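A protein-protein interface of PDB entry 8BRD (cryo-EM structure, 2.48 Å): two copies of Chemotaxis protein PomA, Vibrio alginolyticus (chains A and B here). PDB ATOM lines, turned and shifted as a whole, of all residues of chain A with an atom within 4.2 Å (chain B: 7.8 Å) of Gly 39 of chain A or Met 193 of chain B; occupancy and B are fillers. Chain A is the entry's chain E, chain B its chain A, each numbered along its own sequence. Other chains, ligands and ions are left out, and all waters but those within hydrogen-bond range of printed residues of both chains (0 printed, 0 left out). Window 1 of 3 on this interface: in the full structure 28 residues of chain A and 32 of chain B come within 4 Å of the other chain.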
ATOM      1  N   LEU A  34      20.583  -0.973 -22.376  1.00  0.00           N
ATOM      2  CA  LEU A  34      20.251  -0.504 -23.712  1.00  0.00           C
ATOM      3  C   LEU A  34      20.665   0.948 -23.889  1.00  0.00           C
ATOM      4  O   LEU A  34      21.470   1.265 -24.763  1.00  0.00           O
ATOM      5  CB  LEU A  34      18.757  -0.680 -23.982  1.00  0.00           C
ATOM      6  CG  LEU A  34      18.417  -1.749 -25.021  1.00  0.00           C
ATOM      7  CD1 LEU A  34      19.151  -1.462 -26.322  1.00  0.00           C
ATOM      8  CD2 LEU A  34      18.762  -3.136 -24.503  1.00  0.00           C
ATOM      9  N   ILE A  35      20.205   1.827 -23.002  1.00  0.00           N
ATOM     10  CA  ILE A  35      20.537   3.243 -23.097  1.00  0.00           C
ATOM     11  C   ILE A  35      22.049   3.418 -23.151  1.00  0.00           C
ATOM     12  O   ILE A  35      22.589   3.812 -24.187  1.00  0.00           O
ATOM     13  CB  ILE A  35      19.920   4.044 -21.937  1.00  0.00           C
ATOM     14  CG1 ILE A  35      18.394   4.026 -22.046  1.00  0.00           C
ATOM     15  CG2 ILE A  35      20.439   5.469 -21.935  1.00  0.00           C
ATOM     16  CD1 ILE A  35      17.690   4.670 -20.888  1.00  0.00           C
ATOM     17  N   VAL A  36      22.752   3.030 -22.085  1.00  0.00           N
ATOM     18  CA  VAL A  36      24.180   3.332 -22.009  1.00  0.00           C
ATOM     19  C   VAL A  36      24.948   2.630 -23.123  1.00  0.00           C
ATOM     20  O   VAL A  36      25.556   3.283 -23.979  1.00  0.00           O
ATOM     21  CB  VAL A  36      24.736   2.966 -20.621  1.00  0.00           C
ATOM     22  CG1 VAL A  36      26.231   3.217 -20.572  1.00  0.00           C
ATOM     23  CG2 VAL A  36      24.039   3.774 -19.554  1.00  0.00           C
ATOM     24  N   VAL A  37      24.937   1.297 -23.134  1.00  0.00           N
ATOM     25  CA  VAL A  37      25.735   0.537 -24.082  1.00  0.00           C
ATOM     26  C   VAL A  37      25.311   0.742 -25.534  1.00  0.00           C
ATOM     27  O   VAL A  37      26.179   0.969 -26.387  1.00  0.00           O
ATOM     28  CB  VAL A  37      25.708  -0.964 -23.721  1.00  0.00           C
ATOM     29  CG1 VAL A  37      26.352  -1.797 -24.815  1.00  0.00           C
ATOM     30  CG2 VAL A  37      26.408  -1.195 -22.395  1.00  0.00           C
ATOM     31  N   GLY A  38      24.014   0.660 -25.848  1.00  0.00           N
ATOM     32  CA  GLY A  38      23.568   0.887 -27.206  1.00  0.00           C
ATOM     33  C   GLY A  38      23.800   2.290 -27.716  1.00  0.00           C
ATOM     34  O   GLY A  38      24.201   2.460 -28.869  1.00  0.00           O
ATOM     35  N   GLY A  39      23.557   3.317 -26.896  1.00  0.00           N
ATOM     36  CA  GLY A  39      23.842   4.666 -27.324  1.00  0.00           C
ATOM     37  C   GLY A  39      25.319   4.893 -27.537  1.00  0.00           C
ATOM     38  O   GLY A  39      25.719   5.554 -28.499  1.00  0.00           O
ATOM     39  N   SER A  40      26.147   4.333 -26.650  1.00  0.00           N
ATOM     40  CA  SER A  40      27.590   4.439 -26.821  1.00  0.00           C
ATOM     41  C   SER A  40      28.042   3.745 -28.099  1.00  0.00           C
ATOM     42  O   SER A  40      28.867   4.275 -28.850  1.00  0.00           O
ATOM     43  CB  SER A  40      28.295   3.847 -25.602  1.00  0.00           C
ATOM     44  OG  SER A  40      27.699   4.301 -24.404  1.00  0.00           O
ATOM     45  N   ILE A  41      27.500   2.554 -28.365  1.00  0.00           N
ATOM     46  CA  ILE A  41      27.864   1.811 -29.566  1.00  0.00           C
ATOM     47  C   ILE A  41      27.425   2.563 -30.812  1.00  0.00           C
ATOM     48  O   ILE A  41      28.164   2.641 -31.796  1.00  0.00           O
ATOM     49  CB  ILE A  41      27.269   0.390 -29.514  1.00  0.00           C
ATOM     50  CG1 ILE A  41      28.132  -0.511 -28.632  1.00  0.00           C
ATOM     51  CG2 ILE A  41      27.135  -0.193 -30.908  1.00  0.00           C
ATOM     52  CD1 ILE A  41      27.505  -1.845 -28.328  1.00  0.00           C
ATOM     53  N   PHE A  42      26.220   3.129 -30.790  1.00  0.00           N
ATOM     54  CA  PHE A  42      25.738   3.910 -31.921  1.00  0.00           C
ATOM     55  C   PHE A  42      26.641   5.110 -32.186  1.00  0.00           C
ATOM     56  O   PHE A  42      27.072   5.343 -33.322  1.00  0.00           O
ATOM     57  CB  PHE A  42      24.301   4.349 -31.652  1.00  0.00           C
ATOM     58  CG  PHE A  42      23.826   5.451 -32.540  1.00  0.00           C
ATOM     59  CD1 PHE A  42      23.435   5.189 -33.838  1.00  0.00           C
ATOM     60  CD2 PHE A  42      23.758   6.752 -32.075  1.00  0.00           C
ATOM     61  CE1 PHE A  42      22.997   6.202 -34.651  1.00  0.00           C
ATOM     62  CE2 PHE A  42      23.321   7.765 -32.886  1.00  0.00           C
ATOM     63  CZ  PHE A  42      22.941   7.493 -34.176  1.00  0.00           C
ATOM     64  N   VAL A  43      26.966   5.864 -31.135  1.00  0.00           N
ATOM     65  CA  VAL A  43      27.806   7.047 -31.295  1.00  0.00           C
ATOM     66  C   VAL A  43      29.188   6.664 -31.809  1.00  0.00           C
ATOM     67  O   VAL A  43      29.750   7.340 -32.679  1.00  0.00           O
ATOM     68  CB  VAL A  43      27.881   7.825 -29.968  1.00  0.00           C
ATOM     69  CG1 VAL A  43      29.009   8.831 -29.993  1.00  0.00           C
ATOM     70  CG2 VAL A  43      26.565   8.517 -29.694  1.00  0.00           C
ATOM     71  N   MET A 151      25.677   9.214 -22.101  1.00  0.00           N
ATOM     72  CA  MET A 151      24.509   8.341 -22.131  1.00  0.00           C
ATOM     73  C   MET A 151      23.949   8.113 -20.736  1.00  0.00           C
ATOM     74  O   MET A 151      22.735   7.973 -20.576  1.00  0.00           O
ATOM     75  CB  MET A 151      24.864   7.009 -22.793  1.00  0.00           C
ATOM     76  CG  MET A 151      25.205   7.109 -24.279  1.00  0.00           C
ATOM     77  SD  MET A 151      24.031   7.988 -25.333  1.00  0.00           S
ATOM     78  CE  MET A 151      22.454   7.385 -24.737  1.00  0.00           C
ATOM     79  N   LEU B   7      22.119   1.724 -37.228  1.00  0.00           N
ATOM     80  CA  LEU B   7      21.557   2.965 -36.708  1.00  0.00           C
ATOM     81  C   LEU B   7      20.043   2.872 -36.587  1.00  0.00           C
ATOM     82  O   LEU B   7      19.460   3.232 -35.561  1.00  0.00           O
ATOM     83  CB  LEU B   7      21.962   4.121 -37.633  1.00  0.00           C
ATOM     84  CG  LEU B   7      21.248   5.478 -37.631  1.00  0.00           C
ATOM     85  CD1 LEU B   7      22.233   6.575 -38.001  1.00  0.00           C
ATOM     86  CD2 LEU B   7      20.066   5.502 -38.591  1.00  0.00           C
ATOM     87  N   GLY B  10      19.105   0.328 -33.875  1.00  0.00           N
ATOM     88  CA  GLY B  10      19.354   0.874 -32.553  1.00  0.00           C
ATOM     89  C   GLY B  10      18.346   1.935 -32.167  1.00  0.00           C
ATOM     90  O   GLY B  10      17.880   1.974 -31.028  1.00  0.00           O
ATOM     91  N   PHE B  11      17.999   2.815 -33.108  1.00  0.00           N
ATOM     92  CA  PHE B  11      16.957   3.804 -32.852  1.00  0.00           C
ATOM     93  C   PHE B  11      15.669   3.126 -32.410  1.00  0.00           C
ATOM     94  O   PHE B  11      15.095   3.463 -31.366  1.00  0.00           O
ATOM     95  CB  PHE B  11      16.717   4.652 -34.104  1.00  0.00           C
ATOM     96  CG  PHE B  11      17.640   5.831 -34.232  1.00  0.00           C
ATOM     97  CD1 PHE B  11      18.811   5.898 -33.500  1.00  0.00           C
ATOM     98  CD2 PHE B  11      17.328   6.880 -35.084  1.00  0.00           C
ATOM     99  CE1 PHE B  11      19.655   6.987 -33.615  1.00  0.00           C
ATOM    100  CE2 PHE B  11      18.167   7.971 -35.204  1.00  0.00           C
ATOM    101  CZ  PHE B  11      19.331   8.025 -34.468  1.00  0.00           C
ATOM    102  N   VAL B  14      16.067   1.329 -28.904  1.00  0.00           N
ATOM    103  CA  VAL B  14      16.211   2.231 -27.765  1.00  0.00           C
ATOM    104  C   VAL B  14      14.907   2.969 -27.489  1.00  0.00           C
ATOM    105  O   VAL B  14      14.539   3.176 -26.329  1.00  0.00           O
ATOM    106  CB  VAL B  14      17.391   3.200 -27.976  1.00  0.00           C
ATOM    107  CG1 VAL B  14      17.532   4.119 -26.785  1.00  0.00           C
ATOM    108  CG2 VAL B  14      18.687   2.423 -28.142  1.00  0.00           C
ATOM    109  N   MET B  18      12.910   2.598 -24.053  1.00  0.00           N
ATOM    110  CA  MET B  18      12.673   3.798 -23.260  1.00  0.00           C
ATOM    111  C   MET B  18      11.204   3.970 -22.898  1.00  0.00           C
ATOM    112  O   MET B  18      10.873   4.373 -21.777  1.00  0.00           O
ATOM    113  CB  MET B  18      13.179   5.026 -24.022  1.00  0.00           C
ATOM    114  CG  MET B  18      14.541   5.526 -23.576  1.00  0.00           C
ATOM    115  SD  MET B  18      14.840   7.220 -24.108  1.00  0.00           S
ATOM    116  CE  MET B  18      16.325   7.030 -25.090  1.00  0.00           C
ATOM    117  N   TYR B 186      15.758  16.476 -24.857  1.00  0.00           N
ATOM    118  CA  TYR B 186      15.920  16.573 -26.304  1.00  0.00           C
ATOM    119  C   TYR B 186      17.219  17.269 -26.672  1.00  0.00           C
ATOM    120  O   TYR B 186      17.868  16.893 -27.648  1.00  0.00           O
ATOM    121  CB  TYR B 186      14.739  17.312 -26.923  1.00  0.00           C
ATOM    122  CG  TYR B 186      13.464  16.525 -26.915  1.00  0.00           C
ATOM    123  CD1 TYR B 186      13.446  15.199 -26.505  1.00  0.00           C
ATOM    124  CD2 TYR B 186      12.275  17.102 -27.310  1.00  0.00           C
ATOM    125  CE1 TYR B 186      12.284  14.483 -26.491  1.00  0.00           C
ATOM    126  CE2 TYR B 186      11.108  16.390 -27.303  1.00  0.00           C
ATOM    127  CZ  TYR B 186      11.118  15.083 -26.894  1.00  0.00           C
ATOM    128  OH  TYR B 186       9.946  14.375 -26.887  1.00  0.00           O
ATOM    129  N   GLY B 187      17.594  18.309 -25.930  1.00  0.00           N
ATOM    130  CA  GLY B 187      18.859  18.968 -26.193  1.00  0.00           C
ATOM    131  C   GLY B 187      20.037  18.034 -26.011  1.00  0.00           C
ATOM    132  O   GLY B 187      20.939  17.986 -26.847  1.00  0.00           O
ATOM    133  N   ALA B 188      20.025  17.254 -24.927  1.00  0.00           N
ATOM    134  CA  ALA B 188      21.094  16.284 -24.699  1.00  0.00           C
ATOM    135  C   ALA B 188      21.114  15.207 -25.779  1.00  0.00           C
ATOM    136  O   ALA B 188      22.184  14.841 -26.280  1.00  0.00           O
ATOM    137  CB  ALA B 188      20.945  15.652 -23.318  1.00  0.00           C
ATOM    138  N   ILE B 189      19.942  14.691 -26.155  1.00  0.00           N
ATOM    139  CA  ILE B 189      19.872  13.635 -27.162  1.00  0.00           C
ATOM    140  C   ILE B 189      20.335  14.151 -28.519  1.00  0.00           C
ATOM    141  O   ILE B 189      21.096  13.486 -29.224  1.00  0.00           O
ATOM    142  CB  ILE B 189      18.446  13.055 -27.234  1.00  0.00           C
ATOM    143  CG1 ILE B 189      18.131  12.239 -25.981  1.00  0.00           C
ATOM    144  CG2 ILE B 189      18.272  12.201 -28.477  1.00  0.00           C
ATOM    145  CD1 ILE B 189      16.703  11.779 -25.902  1.00  0.00           C
ATOM    146  N   LEU B 190      19.879  15.342 -28.911  1.00  0.00           N
ATOM    147  CA  LEU B 190      20.279  15.908 -30.193  1.00  0.00           C
ATOM    148  C   LEU B 190      21.764  16.220 -30.216  1.00  0.00           C
ATOM    149  O   LEU B 190      22.432  16.024 -31.237  1.00  0.00           O
ATOM    150  CB  LEU B 190      19.465  17.164 -30.491  1.00  0.00           C
ATOM    151  CG  LEU B 190      18.027  16.964 -30.962  1.00  0.00           C
ATOM    152  CD1 LEU B 190      17.382  18.297 -31.263  1.00  0.00           C
ATOM    153  CD2 LEU B 190      17.990  16.069 -32.179  1.00  0.00           C
ATOM    154  N   SER B 191      22.300  16.718 -29.104  1.00  0.00           N
ATOM    155  CA  SER B 191      23.729  16.977 -29.022  1.00  0.00           C
ATOM    156  C   SER B 191      24.533  15.695 -29.184  1.00  0.00           C
ATOM    157  O   SER B 191      25.423  15.612 -30.034  1.00  0.00           O
ATOM    158  CB  SER B 191      24.047  17.651 -27.690  1.00  0.00           C
ATOM    159  OG  SER B 191      25.441  17.767 -27.490  1.00  0.00           O
ATOM    160  N   ASN B 192      24.213  14.673 -28.393  1.00  0.00           N
ATOM    161  CA  ASN B 192      25.108  13.531 -28.268  1.00  0.00           C
ATOM    162  C   ASN B 192      24.856  12.437 -29.295  1.00  0.00           C
ATOM    163  O   ASN B 192      25.785  11.697 -29.632  1.00  0.00           O
ATOM    164  CB  ASN B 192      25.007  12.947 -26.858  1.00  0.00           C
ATOM    165  CG  ASN B 192      25.636  13.844 -25.822  1.00  0.00           C
ATOM    166  OD1 ASN B 192      26.755  14.317 -25.996  1.00  0.00           O
ATOM    167  ND2 ASN B 192      24.913  14.098 -24.741  1.00  0.00           N
ATOM    168  N   MET B 193      23.636  12.316 -29.809  1.00  0.00           N
ATOM    169  CA  MET B 193      23.282  11.228 -30.702  1.00  0.00           C
ATOM    170  C   MET B 193      22.882  11.683 -32.096  1.00  0.00           C
ATOM    171  O   MET B 193      22.613  10.832 -32.949  1.00  0.00           O
ATOM    172  CB  MET B 193      22.143  10.395 -30.097  1.00  0.00           C
ATOM    173  CG  MET B 193      22.234  10.221 -28.593  1.00  0.00           C
ATOM    174  SD  MET B 193      21.376   8.750 -28.027  1.00  0.00           S
ATOM    175  CE  MET B 193      22.246   7.491 -28.949  1.00  0.00           C
ATOM    176  N   VAL B 194      22.818  12.988 -32.357  1.00  0.00           N
ATOM    177  CA  VAL B 194      22.517  13.451 -33.708  1.00  0.00           C
ATOM    178  C   VAL B 194      23.612  14.380 -34.220  1.00  0.00           C
ATOM    179  O   VAL B 194      24.326  14.038 -35.165  1.00  0.00           O
ATOM    180  CB  VAL B 194      21.144  14.142 -33.766  1.00  0.00           C
ATOM    181  CG1 VAL B 194      20.865  14.631 -35.171  1.00  0.00           C
ATOM    182  CG2 VAL B 194      20.054  13.194 -33.312  1.00  0.00           C
ATOM    183  N   PHE B 195      23.776  15.543 -33.591  1.00  0.00           N
ATOM    184  CA  PHE B 195      24.617  16.588 -34.173  1.00  0.00           C
ATOM    185  C   PHE B 195      26.099  16.244 -34.096  1.00  0.00           C
ATOM    186  O   PHE B 195      26.822  16.362 -35.089  1.00  0.00           O
ATOM    187  CB  PHE B 195      24.347  17.925 -33.487  1.00  0.00           C
ATOM    188  CG  PHE B 195      23.012  18.509 -33.816  1.00  0.00           C
ATOM    189  CD1 PHE B 195      22.530  18.474 -35.110  1.00  0.00           C
ATOM    190  CD2 PHE B 195      22.236  19.085 -32.832  1.00  0.00           C
ATOM    191  CE1 PHE B 195      21.300  19.008 -35.416  1.00  0.00           C
ATOM    192  CE2 PHE B 195      21.005  19.619 -33.131  1.00  0.00           C
ATOM    193  CZ  PHE B 195      20.536  19.581 -34.425  1.00  0.00           C
ATOM    194  N   PHE B 196      26.572  15.841 -32.925  1.00  0.00           N
ATOM    195  CA  PHE B 196      27.963  15.438 -32.764  1.00  0.00           C
ATOM    196  C   PHE B 196      28.275  14.186 -33.583  1.00  0.00           C
ATOM    197  O   PHE B 196      29.348  14.116 -34.193  1.00  0.00           O
ATOM    198  CB  PHE B 196      28.300  15.229 -31.286  1.00  0.00           C
ATOM    199  CG  PHE B 196      28.532  16.506 -30.533  1.00  0.00           C
ATOM    200  CD1 PHE B 196      29.059  17.615 -31.170  1.00  0.00           C
ATOM    201  CD2 PHE B 196      28.223  16.601 -29.189  1.00  0.00           C
ATOM    202  CE1 PHE B 196      29.275  18.788 -30.481  1.00  0.00           C
ATOM    203  CE2 PHE B 196      28.434  17.773 -28.497  1.00  0.00           C
ATOM    204  CZ  PHE B 196      28.962  18.864 -29.141  1.00  0.00           C
ATOM    205  N   PRO B 197      27.405  13.164 -33.599  1.00  0.00           N
ATOM    206  CA  PRO B 197      27.635  12.053 -34.538  1.00  0.00           C
ATOM    207  C   PRO B 197      27.666  12.473 -35.998  1.00  0.00           C
ATOM    208  O   PRO B 197      28.457  11.921 -36.767  1.00  0.00           O
ATOM    209  CB  PRO B 197      26.462  11.114 -34.242  1.00  0.00           C
ATOM    210  CG  PRO B 197      26.179  11.346 -32.836  1.00  0.00           C
ATOM    211  CD  PRO B 197      26.344  12.818 -32.637  1.00  0.00           C
ATOM    212  N   ILE B 198      26.828  13.427 -36.407  1.00  0.00           N
ATOM    213  CA  ILE B 198      26.871  13.902 -37.788  1.00  0.00           C
ATOM    214  C   ILE B 198      28.196  14.599 -38.065  1.00  0.00           C
ATOM    215  O   ILE B 198      28.788  14.435 -39.138  1.00  0.00           O
ATOM    216  CB  ILE B 198      25.674  14.819 -38.086  1.00  0.00           C
ATOM    217  CG1 ILE B 198      24.393  14.001 -38.222  1.00  0.00           C
ATOM    218  CG2 ILE B 198      25.908  15.598 -39.365  1.00  0.00           C
ATOM    219  CD1 ILE B 198      23.204  14.807 -38.679  1.00  0.00           C
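The backbone carbonyl oxygen (O) of Ala 188 of chain B lies within hydrogen-bond range of the side-chain amide nitrogen (ND2) of Asn 192 of chain B.
No position is printed for both chains.
Of the 6 pairs that touch across the chains among the printed residues, none has its exchanged pair printed and touching as well.
Gly 39 of chain A touches just one residue of chain B: Met 193.
Printed residues of chain B within 4 Å of Phe 42 of chain A: Leu 7, Phe 11 and Met 193.
Printed residues of chain A within 4 Å of Leu 7 of chain B: Phe 42 (3.5 Å).
Of the printed residues of chain A, Asn 192 of chain B touches Val 43 (3.3 Å).
Met 193 of chain B touches just these residues of chain A: Gly 39 (3.6 Å), Phe 42 (3.1 Å) and Met 151 (3.7 Å).
The nearest residue of chain B that does not touch Gly 39 of chain A is Val 14 of chain B (5.1 Å).
Of the 11 printed residues of chain A, 4 touch a printed residue of chain B.
Hydrophobic or aromatic side chains of chain B that line the printed part of chain A: Leu 7, Phe 11 and Met 193.
Among the printed residues, 6 pairs touch across the chains.
Among the printed residues, pairs that only touch across the chains: Gly 39 of chain A with Met 193 of chain B (3.6 Å), Phe 42 of chain A with Leu 7 of chain B (3.5 Å), Phe 42 of chain A with Phe 11 of chain B (3.4 Å), Phe 42 of chain A with Met 193 of chain B (3.1 Å), Val 43 of chain A with Asn 192 of chain B (3.3 Å) and Met 151 of chain A with Met 193 of chain B (3.7 Å).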
